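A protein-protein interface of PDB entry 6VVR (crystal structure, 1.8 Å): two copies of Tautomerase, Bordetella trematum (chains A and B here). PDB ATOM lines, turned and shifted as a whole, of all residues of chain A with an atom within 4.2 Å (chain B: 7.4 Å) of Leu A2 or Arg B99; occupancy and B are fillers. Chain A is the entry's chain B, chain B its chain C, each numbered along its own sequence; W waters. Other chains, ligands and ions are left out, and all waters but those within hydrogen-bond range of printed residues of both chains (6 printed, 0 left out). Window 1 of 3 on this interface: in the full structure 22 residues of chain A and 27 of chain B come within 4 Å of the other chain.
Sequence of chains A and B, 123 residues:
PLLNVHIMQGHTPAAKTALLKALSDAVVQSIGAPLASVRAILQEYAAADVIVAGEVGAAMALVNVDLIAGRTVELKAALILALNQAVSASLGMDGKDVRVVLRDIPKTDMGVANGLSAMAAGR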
ATOM      1  N   PRO A   1       9.946   4.331  14.426  1.00  0.00           N
ATOM      2  CA  PRO A   1      10.546   5.378  15.263  1.00  0.00           C
ATOM      3  C   PRO A   1       9.581   6.537  15.500  1.00  0.00           C
ATOM      4  O   PRO A   1       8.873   6.966  14.580  1.00  0.00           O
ATOM      5  CB  PRO A   1      11.760   5.831  14.446  1.00  0.00           C
ATOM      6  CG  PRO A   1      12.131   4.604  13.634  1.00  0.00           C
ATOM      7  CD  PRO A   1      10.793   3.997  13.268  1.00  0.00           C
ATOM      8  N   LEU A   2       9.556   7.038  16.728  1.00  0.00           N
ATOM      9  CA  LEU A   2       8.662   8.123  17.110  1.00  0.00           C
ATOM     10  C   LEU A   2       9.517   9.348  17.401  1.00  0.00           C
ATOM     11  O   LEU A   2      10.365   9.334  18.300  1.00  0.00           O
ATOM     12  CB  LEU A   2       7.806   7.720  18.311  1.00  0.00           C
ATOM     13  CG  LEU A   2       7.051   6.396  18.103  1.00  0.00           C
ATOM     14  CD1 LEU A   2       6.271   5.982  19.348  1.00  0.00           C
ATOM     15  CD2 LEU A   2       6.102   6.531  16.926  1.00  0.00           C
ATOM     16  N   LEU A   3       9.328  10.386  16.609  1.00  0.00           N
ATOM     17  CA  LEU A   3      10.121  11.596  16.714  1.00  0.00           C
ATOM     18  C   LEU A   3       9.314  12.680  17.399  1.00  0.00           C
ATOM     19  O   LEU A   3       8.135  12.866  17.098  1.00  0.00           O
ATOM     20  CB  LEU A   3      10.543  12.092  15.330  1.00  0.00           C
ATOM     21  CG  LEU A   3      11.746  11.421  14.677  1.00  0.00           C
ATOM     22  CD1 LEU A   3      11.575   9.919  14.513  1.00  0.00           C
ATOM     23  CD2 LEU A   3      12.083  12.092  13.338  1.00  0.00           C
ATOM     24  N   ASN A   4       9.946  13.405  18.313  1.00  0.00           N
ATOM     25  CA  ASN A   4       9.393  14.673  18.766  1.00  0.00           C
ATOM     26  C   ASN A   4      10.453  15.734  18.523  1.00  0.00           C
ATOM     27  O   ASN A   4      11.602  15.588  18.952  1.00  0.00           O
ATOM     28  CB  ASN A   4       8.908  14.661  20.224  1.00  0.00           C
ATOM     29  CG  ASN A   4       9.945  14.200  21.208  1.00  0.00           C
ATOM     30  OD1 ASN A   4      10.650  15.019  21.813  1.00  0.00           O
ATOM     31  ND2 ASN A   4       9.990  12.891  21.451  1.00  0.00           N
ATOM     32  N   ARG A  39       6.611   8.303  12.933  1.00  0.00           N
ATOM     33  CA  ARG A  39       5.787   9.445  13.317  1.00  0.00           C
ATOM     34  C   ARG A  39       6.695  10.561  13.798  1.00  0.00           C
ATOM     35  O   ARG A  39       7.745  10.309  14.398  1.00  0.00           O
ATOM     36  CB  ARG A  39       4.802   9.104  14.434  1.00  0.00           C
ATOM     37  CG  ARG A  39       4.045   7.817  14.204  1.00  0.00           C
ATOM     38  CD  ARG A  39       3.034   7.501  15.304  1.00  0.00           C
ATOM     39  NE  ARG A  39       2.130   6.478  14.795  1.00  0.00           N
ATOM     40  CZ  ARG A  39       0.846   6.378  15.100  1.00  0.00           C
ATOM     41  NH1 ARG A  39       0.290   7.226  15.957  1.00  0.00           N
ATOM     42  NH2 ARG A  39       0.118   5.425  14.534  1.00  0.00           N
ATOM     43  N   ASN A  64      14.330  14.421  19.000  1.00  0.00           N
ATOM     44  CA  ASN A  64      14.387  13.274  19.902  1.00  0.00           C
ATOM     45  C   ASN A  64      13.735  12.076  19.232  1.00  0.00           C
ATOM     46  O   ASN A  64      12.601  12.173  18.757  1.00  0.00           O
ATOM     47  CB  ASN A  64      13.665  13.560  21.218  1.00  0.00           C
ATOM     48  CG  ASN A  64      14.377  14.590  22.048  1.00  0.00           C
ATOM     49  OD1 ASN A  64      15.597  14.745  21.955  1.00  0.00           O
ATOM     50  ND2 ASN A  64      13.625  15.302  22.868  1.00  0.00           N
ATOM     51  N   VAL A  65      14.432  10.947  19.218  1.00  0.00           N
ATOM     52  CA  VAL A  65      13.953   9.744  18.545  1.00  0.00           C
ATOM     53  C   VAL A  65      13.835   8.626  19.565  1.00  0.00           C
ATOM     54  O   VAL A  65      14.845   8.211  20.141  1.00  0.00           O
ATOM     55  CB  VAL A  65      14.896   9.311  17.412  1.00  0.00           C
ATOM     56  CG1 VAL A  65      14.280   8.128  16.668  1.00  0.00           C
ATOM     57  CG2 VAL A  65      15.208  10.487  16.476  1.00  0.00           C
ATOM     58  N   ASP A  66      12.615   8.115  19.764  1.00  0.00           N
ATOM     59  CA  ASP A  66      12.403   6.865  20.484  1.00  0.00           C
ATOM     60  C   ASP A  66      12.225   5.771  19.434  1.00  0.00           C
ATOM     61  O   ASP A  66      11.278   5.813  18.637  1.00  0.00           O
ATOM     62  CB  ASP A  66      11.191   6.948  21.417  1.00  0.00           C
ATOM     63  CG  ASP A  66      11.367   7.990  22.515  1.00  0.00           C
ATOM     64  OD1 ASP A  66      12.462   8.062  23.103  1.00  0.00           O
ATOM     65  OD2 ASP A  66      10.412   8.753  22.788  1.00  0.00           O
ATOM     66  N   MET A 110       8.114  -0.834  23.982  1.00  0.00           N
ATOM     67  CA  MET A 110       7.570  -0.001  22.918  1.00  0.00           C
ATOM     68  C   MET A 110       6.145  -0.440  22.615  1.00  0.00           C
ATOM     69  O   MET A 110       5.926  -1.564  22.154  1.00  0.00           O
ATOM     70  CB  MET A 110       8.434  -0.099  21.660  1.00  0.00           C
ATOM     71  CG  MET A 110       7.855   0.666  20.481  1.00  0.00           C
ATOM     72  SD  MET A 110       7.988   2.453  20.735  1.00  0.00           S
ATOM     73  CE  MET A 110       9.747   2.661  20.526  1.00  0.00           C
ATOM     74  N   GLY A 111       5.185   0.445  22.865  1.00  0.00           N
ATOM     75  CA  GLY A 111       3.818   0.161  22.498  1.00  0.00           C
ATOM     76  C   GLY A 111       3.601   0.361  21.007  1.00  0.00           C
ATOM     77  O   GLY A 111       4.182   1.249  20.378  1.00  0.00           O
ATOM     78  N   VAL A 112       2.761  -0.493  20.438  1.00  0.00           N
ATOM     79  CA  VAL A 112       2.349  -0.306  19.053  1.00  0.00           C
ATOM     80  C   VAL A 112       0.836  -0.108  19.053  1.00  0.00           C
ATOM     81  O   VAL A 112       0.249   0.276  20.076  1.00  0.00           O
ATOM     82  CB  VAL A 112       2.797  -1.485  18.164  1.00  0.00           C
ATOM     83  CG1 VAL A 112       4.328  -1.511  18.053  1.00  0.00           C
ATOM     84  CG2 VAL A 112       2.289  -2.805  18.716  1.00  0.00           C
ATOM     85  N   ALA A 113       0.196  -0.359  17.913  1.00  0.00           N
ATOM     86  CA  ALA A 113      -1.238  -0.125  17.807  1.00  0.00           C
ATOM     87  C   ALA A 113      -1.999  -0.892  18.884  1.00  0.00           C
ATOM     88  O   ALA A 113      -1.647  -2.023  19.234  1.00  0.00           O
ATOM     89  CB  ALA A 113      -1.739  -0.535  16.421  1.00  0.00           C
ATOM     90  N   HIS B   6       0.726  13.650  24.692  1.00  0.00           N
ATOM     91  CA  HIS B   6       0.724  14.498  23.508  1.00  0.00           C
ATOM     92  C   HIS B   6      -0.521  14.150  22.715  1.00  0.00           C
ATOM     93  O   HIS B   6      -0.666  13.009  22.268  1.00  0.00           O
ATOM     94  CB  HIS B   6       1.988  14.266  22.688  1.00  0.00           C
ATOM     95  CG  HIS B   6       3.240  14.375  23.495  1.00  0.00           C
ATOM     96  ND1 HIS B   6       3.971  15.539  23.575  1.00  0.00           N
ATOM     97  CD2 HIS B   6       3.868  13.478  24.291  1.00  0.00           C
ATOM     98  CE1 HIS B   6       5.011  15.345  24.368  1.00  0.00           C
ATOM     99  NE2 HIS B   6       4.968  14.106  24.820  1.00  0.00           N
ATOM    100  N   VAL B  52       2.239  11.258  10.355  1.00  0.00           N
ATOM    101  CA  VAL B  52       2.136   9.856  10.746  1.00  0.00           C
ATOM    102  C   VAL B  52       2.184   9.025   9.470  1.00  0.00           C
ATOM    103  O   VAL B  52       1.342   9.205   8.586  1.00  0.00           O
ATOM    104  CB  VAL B  52       0.846   9.559  11.539  1.00  0.00           C
ATOM    105  CG1 VAL B  52       0.721   8.064  11.816  1.00  0.00           C
ATOM    106  CG2 VAL B  52       0.804  10.342  12.862  1.00  0.00           C
ATOM    107  N   MET B  60      -2.998  11.775  16.015  1.00  0.00           N
ATOM    108  CA  MET B  60      -2.200  10.854  16.811  1.00  0.00           C
ATOM    109  C   MET B  60      -2.354  11.224  18.276  1.00  0.00           C
ATOM    110  O   MET B  60      -2.724  12.347  18.616  1.00  0.00           O
ATOM    111  CB  MET B  60      -0.712  10.898  16.411  1.00  0.00           C
ATOM    112  CG  MET B  60      -0.001  12.214  16.791  1.00  0.00           C
ATOM    113  SD  MET B  60       0.617  12.264  18.491  1.00  0.00           S
ATOM    114  CE  MET B  60       0.327  13.972  18.941  1.00  0.00           C
ATOM    115  N   ALA B  61      -2.049  10.262  19.142  1.00  0.00           N
ATOM    116  CA  ALA B  61      -1.809  10.541  20.548  1.00  0.00           C
ATOM    117  C   ALA B  61      -0.584   9.745  20.971  1.00  0.00           C
ATOM    118  O   ALA B  61      -0.313   8.673  20.427  1.00  0.00           O
ATOM    119  CB  ALA B  61      -3.020  10.188  21.434  1.00  0.00           C
ATOM    120  N   LEU B  62       0.177  10.298  21.918  1.00  0.00           N
ATOM    121  CA  LEU B  62       1.414   9.672  22.364  1.00  0.00           C
ATOM    122  C   LEU B  62       1.519   9.813  23.870  1.00  0.00           C
ATOM    123  O   LEU B  62       1.336  10.911  24.407  1.00  0.00           O
ATOM    124  CB  LEU B  62       2.644  10.308  21.686  1.00  0.00           C
ATOM    125  CG  LEU B  62       4.031   9.856  22.168  1.00  0.00           C
ATOM    126  CD1 LEU B  62       4.317   8.392  21.767  1.00  0.00           C
ATOM    127  CD2 LEU B  62       5.116  10.780  21.602  1.00  0.00           C
ATOM    128  N   VAL B  63       1.811   8.711  24.547  1.00  0.00           N
ATOM    129  CA  VAL B  63       2.032   8.712  25.987  1.00  0.00           C
ATOM    130  C   VAL B  63       3.455   8.247  26.222  1.00  0.00           C
ATOM    131  O   VAL B  63       3.767   7.066  26.018  1.00  0.00           O
ATOM    132  CB  VAL B  63       1.048   7.804  26.733  1.00  0.00           C
ATOM    133  CG1 VAL B  63       1.297   7.910  28.231  1.00  0.00           C
ATOM    134  CG2 VAL B  63      -0.387   8.179  26.392  1.00  0.00           C
ATOM    135  N   ASN B  64       4.312   9.157  26.670  1.00  0.00           N
ATOM    136  CA  ASN B  64       5.680   8.816  27.040  1.00  0.00           C
ATOM    137  C   ASN B  64       5.757   8.642  28.548  1.00  0.00           C
ATOM    138  O   ASN B  64       5.296   9.510  29.297  1.00  0.00           O
ATOM    139  CB  ASN B  64       6.660   9.895  26.587  1.00  0.00           C
ATOM    140  CG  ASN B  64       6.825   9.937  25.076  1.00  0.00           C
ATOM    141  OD1 ASN B  64       6.688   8.923  24.391  1.00  0.00           O
ATOM    142  ND2 ASN B  64       7.124  11.114  24.553  1.00  0.00           N
ATOM    143  N   ILE B  80       1.082  -0.699  29.294  1.00  0.00           N
ATOM    144  CA  ILE B  80       0.913  -0.205  27.931  1.00  0.00           C
ATOM    145  C   ILE B  80      -0.545  -0.327  27.503  1.00  0.00           C
ATOM    146  O   ILE B  80      -1.129   0.611  26.943  1.00  0.00           O
ATOM    147  CB  ILE B  80       1.861  -0.966  26.984  1.00  0.00           C
ATOM    148  CG1 ILE B  80       3.313  -0.585  27.288  1.00  0.00           C
ATOM    149  CG2 ILE B  80       1.538  -0.675  25.538  1.00  0.00           C
ATOM    150  CD1 ILE B  80       4.349  -1.453  26.583  1.00  0.00           C
ATOM    151  N   LEU B  83      -2.837   2.220  29.489  1.00  0.00           N
ATOM    152  CA  LEU B  83      -2.691   3.608  29.058  1.00  0.00           C
ATOM    153  C   LEU B  83      -3.328   3.829  27.692  1.00  0.00           C
ATOM    154  O   LEU B  83      -3.954   4.871  27.454  1.00  0.00           O
ATOM    155  CB  LEU B  83      -1.216   4.003  29.016  1.00  0.00           C
ATOM    156  CG  LEU B  83      -0.503   4.001  30.364  1.00  0.00           C
ATOM    157  CD1 LEU B  83       0.994   4.249  30.153  1.00  0.00           C
ATOM    158  CD2 LEU B  83      -1.106   5.033  31.292  1.00  0.00           C
ATOM    159  N   ASN B  84      -3.160   2.871  26.778  1.00  0.00           N
ATOM    160  CA  ASN B  84      -3.790   2.989  25.465  1.00  0.00           C
ATOM    161  C   ASN B  84      -5.307   3.065  25.610  1.00  0.00           C
ATOM    162  O   ASN B  84      -5.967   3.918  25.003  1.00  0.00           O
ATOM    163  CB  ASN B  84      -3.376   1.804  24.582  1.00  0.00           C
ATOM    164  CG  ASN B  84      -3.768   1.987  23.111  1.00  0.00           C
ATOM    165  OD1 ASN B  84      -2.909   2.263  22.245  1.00  0.00           O
ATOM    166  ND2 ASN B  84      -5.049   1.817  22.819  1.00  0.00           N
ATOM    167  N   VAL B  87      -6.426   6.519  26.917  1.00  0.00           N
ATOM    168  CA  VAL B  87      -6.496   7.535  25.872  1.00  0.00           C
ATOM    169  C   VAL B  87      -7.707   7.285  24.982  1.00  0.00           C
ATOM    170  O   VAL B  87      -8.507   8.188  24.721  1.00  0.00           O
ATOM    171  CB  VAL B  87      -5.201   7.545  25.043  1.00  0.00           C
ATOM    172  CG1 VAL B  87      -5.323   8.533  23.893  1.00  0.00           C
ATOM    173  CG2 VAL B  87      -4.008   7.859  25.926  1.00  0.00           C
ATOM    174  N   MET B  93     -10.863   8.087  20.587  1.00  0.00           N
ATOM    175  CA  MET B  93      -9.931   7.733  19.527  1.00  0.00           C
ATOM    176  C   MET B  93      -9.865   6.227  19.330  1.00  0.00           C
ATOM    177  O   MET B  93     -10.130   5.443  20.246  1.00  0.00           O
ATOM    178  CB  MET B  93      -8.521   8.222  19.851  1.00  0.00           C
ATOM    179  CG  MET B  93      -8.352   9.687  20.062  1.00  0.00           C
ATOM    180  SD  MET B  93      -6.600   9.976  20.371  1.00  0.00           S
ATOM    181  CE  MET B  93      -5.868   9.427  18.832  1.00  0.00           C
ATOM    182  N   ASP B  94      -9.445   5.831  18.128  1.00  0.00           N
ATOM    183  CA  ASP B  94      -9.092   4.442  17.873  1.00  0.00           C
ATOM    184  C   ASP B  94      -7.717   4.147  18.455  1.00  0.00           C
ATOM    185  O   ASP B  94      -6.765   4.918  18.255  1.00  0.00           O
ATOM    186  CB  ASP B  94      -9.109   4.135  16.376  1.00  0.00           C
ATOM    187  CG  ASP B  94     -10.464   4.391  15.743  1.00  0.00           C
ATOM    188  OD1 ASP B  94     -11.481   4.313  16.463  1.00  0.00           O
ATOM    189  OD2 ASP B  94     -10.514   4.688  14.527  1.00  0.00           O
ATOM    190  N   GLY B  95      -7.617   3.023  19.172  1.00  0.00           N
ATOM    191  CA  GLY B  95      -6.356   2.599  19.746  1.00  0.00           C
ATOM    192  C   GLY B  95      -5.231   2.453  18.741  1.00  0.00           C
ATOM    193  O   GLY B  95      -4.058   2.506  19.118  1.00  0.00           O
ATOM    194  N   LYS B  96      -5.560   2.278  17.457  1.00  0.00           N
ATOM    195  CA  LYS B  96      -4.510   2.191  16.453  1.00  0.00           C
ATOM    196  C   LYS B  96      -3.807   3.523  16.227  1.00  0.00           C
ATOM    197  O   LYS B  96      -2.694   3.541  15.687  1.00  0.00           O
ATOM    198  CB  LYS B  96      -5.074   1.664  15.125  1.00  0.00           C
ATOM    199  CG  LYS B  96      -5.900   2.650  14.333  1.00  0.00           C
ATOM    200  CD  LYS B  96      -6.071   2.153  12.888  1.00  0.00           C
ATOM    201  CE  LYS B  96      -6.987   3.053  12.079  1.00  0.00           C
ATOM    202  NZ  LYS B  96      -6.491   4.457  12.035  1.00  0.00           N
ATOM    203  N   ASP B  97      -4.413   4.627  16.647  1.00  0.00           N
ATOM    204  CA  ASP B  97      -3.829   5.951  16.500  1.00  0.00           C
ATOM    205  C   ASP B  97      -3.065   6.395  17.739  1.00  0.00           C
ATOM    206  O   ASP B  97      -2.558   7.523  17.769  1.00  0.00           O
ATOM    207  CB  ASP B  97      -4.919   6.969  16.160  1.00  0.00           C
ATOM    208  CG  ASP B  97      -5.587   6.666  14.840  1.00  0.00           C
ATOM    209  OD1 ASP B  97      -4.901   6.097  13.970  1.00  0.00           O
ATOM    210  OD2 ASP B  97      -6.780   6.985  14.669  1.00  0.00           O
ATOM    211  N   VAL B  98      -2.959   5.533  18.748  1.00  0.00           N
ATOM    212  CA  VAL B  98      -2.307   5.851  20.013  1.00  0.00           C
ATOM    213  C   VAL B  98      -1.004   5.066  20.110  1.00  0.00           C
ATOM    214  O   VAL B  98      -0.933   3.902  19.689  1.00  0.00           O
ATOM    215  CB  VAL B  98      -3.232   5.526  21.203  1.00  0.00           C
ATOM    216  CG1 VAL B  98      -2.540   5.827  22.533  1.00  0.00           C
ATOM    217  CG2 VAL B  98      -4.565   6.285  21.081  1.00  0.00           C
ATOM    218  N   ARG B  99       0.030   5.697  20.667  1.00  0.00           N
ATOM    219  CA  ARG B  99       1.283   5.007  20.949  1.00  0.00           C
ATOM    220  C   ARG B  99       1.699   5.288  22.383  1.00  0.00           C
ATOM    221  O   ARG B  99       1.494   6.388  22.897  1.00  0.00           O
ATOM    222  CB  ARG B  99       2.414   5.425  19.991  1.00  0.00           C
ATOM    223  CG  ARG B  99       2.252   4.912  18.557  1.00  0.00           C
ATOM    224  CD  ARG B  99       2.190   3.381  18.508  1.00  0.00           C
ATOM    225  NE  ARG B  99       2.086   2.892  17.130  1.00  0.00           N
ATOM    226  CZ  ARG B  99       0.949   2.816  16.440  1.00  0.00           C
ATOM    227  NH1 ARG B  99       0.958   2.361  15.186  1.00  0.00           N
ATOM    228  NH2 ARG B  99      -0.199   3.181  16.997  1.00  0.00           N
ATOM    229  N   VAL B 100       2.277   4.275  23.020  1.00  0.00           N
ATOM    230  CA  VAL B 100       2.792   4.355  24.382  1.00  0.00           C
ATOM    231  C   VAL B 100       4.262   3.970  24.336  1.00  0.00           C
ATOM    232  O   VAL B 100       4.613   2.945  23.746  1.00  0.00           O
ATOM    233  CB  VAL B 100       2.030   3.407  25.329  1.00  0.00           C
ATOM    234  CG1 VAL B 100       2.689   3.381  26.692  1.00  0.00           C
ATOM    235  CG2 VAL B 100       0.559   3.806  25.418  1.00  0.00           C
ATOM    236  N   VAL B 101       5.121   4.781  24.946  1.00  0.00           N
ATOM    237  CA  VAL B 101       6.544   4.469  25.027  1.00  0.00           C
ATOM    238  C   VAL B 101       6.944   4.458  26.493  1.00  0.00           C
ATOM    239  O   VAL B 101       6.778   5.465  27.191  1.00  0.00           O
ATOM    240  CB  VAL B 101       7.403   5.477  24.244  1.00  0.00           C
ATOM    241  CG1 VAL B 101       8.876   5.103  24.364  1.00  0.00           C
ATOM    242  CG2 VAL B 101       6.962   5.527  22.778  1.00  0.00           C
ATOM    243  N   ARG B 103      10.094   4.248  29.092  1.00  0.00           N
ATOM    244  CA  ARG B 103      11.539   4.424  29.231  1.00  0.00           C
ATOM    245  C   ARG B 103      11.949   3.969  30.630  1.00  0.00           C
ATOM    246  O   ARG B 103      11.623   4.629  31.623  1.00  0.00           O
ATOM    247  CB  ARG B 103      11.940   5.877  28.977  1.00  0.00           C
ATOM    248  CG  ARG B 103      11.453   6.394  27.630  1.00  0.00           C
ATOM    249  CD  ARG B 103      12.226   7.617  27.192  1.00  0.00           C
ATOM    250  NE  ARG B 103      11.551   8.337  26.115  1.00  0.00           N
ATOM    251  CZ  ARG B 103      10.752   9.377  26.311  1.00  0.00           C
ATOM    252  NH1 ARG B 103      10.199   9.992  25.271  1.00  0.00           N
ATOM    253  NH2 ARG B 103      10.527   9.809  27.551  1.00  0.00           N
HETATM  254  O   HOH W   1       1.658   8.517  18.314  1.00  0.00           O
HETATM  255  O   HOH W   2      11.070  13.056  24.441  1.00  0.00           O
HETATM  256  O   HOH W   3       8.115   9.017  22.023  1.00  0.00           O
HETATM  257  O   HOH W   4       3.519   4.304  13.869  1.00  0.00           O
HETATM  258  O   HOH W   5      -2.120   7.870  14.180  1.00  0.00           O
HETATM  259  O   HOH W   6       0.856   1.692  22.181  1.00  0.00           O
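The backbone carbonyl oxygen of Asp A66 lies within hydrogen-bond range of the backbone NH of Leu A2, at 2.8 Å.
OD1 of Asn B84 lies close to O of Gly B95.
OD1 of Asp B97 is in salt-bridge range of NZ of Lys B96 (3.0 Å).
O of Arg B99 is in hydrogen-bond range of N of Val B63, at 2.9 Å.
O of Lys B96 lies within hydrogen-bond range of NH2 of Arg B99 (2.8 Å).
The backbone carbonyl oxygen (O) of Ala B61 is in hydrogen-bond range of the backbone NH (N) of Arg B99.
Of chain A, only Leu A2, Arg A39, Gly A111, Val A112 and Ala A113 come within 4 Å of Arg B99.
Of the printed residues of chain B, Val A112 touches Val B98 and Arg B99.
Of the printed residues of chain B, Gly A111 touches Ile B80, Arg B99 and Val B100.
Printed residues of chain B within 4 Å of Asp A66: Arg B103 (2.8 Å).
Of the printed residues of chain A, Arg B103 touches Asp A66 (2.8 Å).
Val B63 touches none of the printed residues of chain A.
Asn A4 touches none of the printed residues of chain B.
1 position is printed for both chains.
Of the 19 pairs that touch across the chains among the printed residues, none has its exchanged pair printed and touching as well.
Water W3 bridges OD2 of Asp A66 (2.4 Å) and OD1 of Asn B64 (2.8 Å).
Water W6 bridges O of Val A112 (2.6 Å) and N of Val B100 (3.1 Å).
Water W4 bridges the guanidinium group of Arg A39 and the guanidinium group of Arg B99.
Water W1 bridges O of Ala B61 and NH1 of Arg A39.
Water W5 bridges the guanidinium group (NH1) of Arg A39 (3.1 Å) and the side-chain carboxylate (OD1) of Asp B97 (3.3 Å).
Water W2 lies within hydrogen-bond range of ND2 of Asn A4 (3.2 Å) and NH1 of Arg B103 (3.3 Å).
Leu A2 touches Arg B99 (CD1 to CB, 3.9 Å).
Leu A2 touches Val B101 (CD1 to CG2, 3.5 Å).
Arg A39 touches Val B52.
Arg A39 touches Met B60 (NH1 to CB, 3.8 Å).
O of Lys B96 touches NH2 of Arg A39, at 3.6 Å.
Gly A111 touches Ile B80 (CA to CG2, 3.9 Å).
Arg B99 touches Gly A111 (CD to O, 3.5 Å).
CD of Arg B99 touches CA of Val A112, 3.7 Å away.
C of Ala A113 touches O of Gly B95 (3.98 Å).
CA of Ala A113 touches NH2 of Arg B99, at 3.6 Å.
Of the 12 printed residues of chain A, 7 touch a printed residue of chain B.
Printed residues of chain A that touch a printed residue of chain B: Leu A2, Arg A39, Asp A66, Met A110, Gly A111, Val A112 and Ala A113.
Among the printed residues, 19 pairs touch across the chains.
Among the printed residues, Asp or Glu carboxylates within 4 Å of a Lys or Arg side-chain nitrogen of the other chain: Asp A66 with Arg B103 (2.8 Å).
The backbone carbonyl oxygen (O) of Asp B97 is in hydrogen-bond range of the guanidinium group (NH1) of Arg A39 (3.4 Å).
NH1 of Arg B99 sits close to NH2 of Arg A39 (3.2 Å).
The side-chain carboxylate (OD2) of Asp A66 is in salt-bridge range of the guanidinium group (NH1) of Arg B103 (2.8 Å).
The backbone NH (N) of Gly A111 lies within hydrogen-bond range of the backbone carbonyl oxygen (O) of Val B100, 2.7 Å away.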
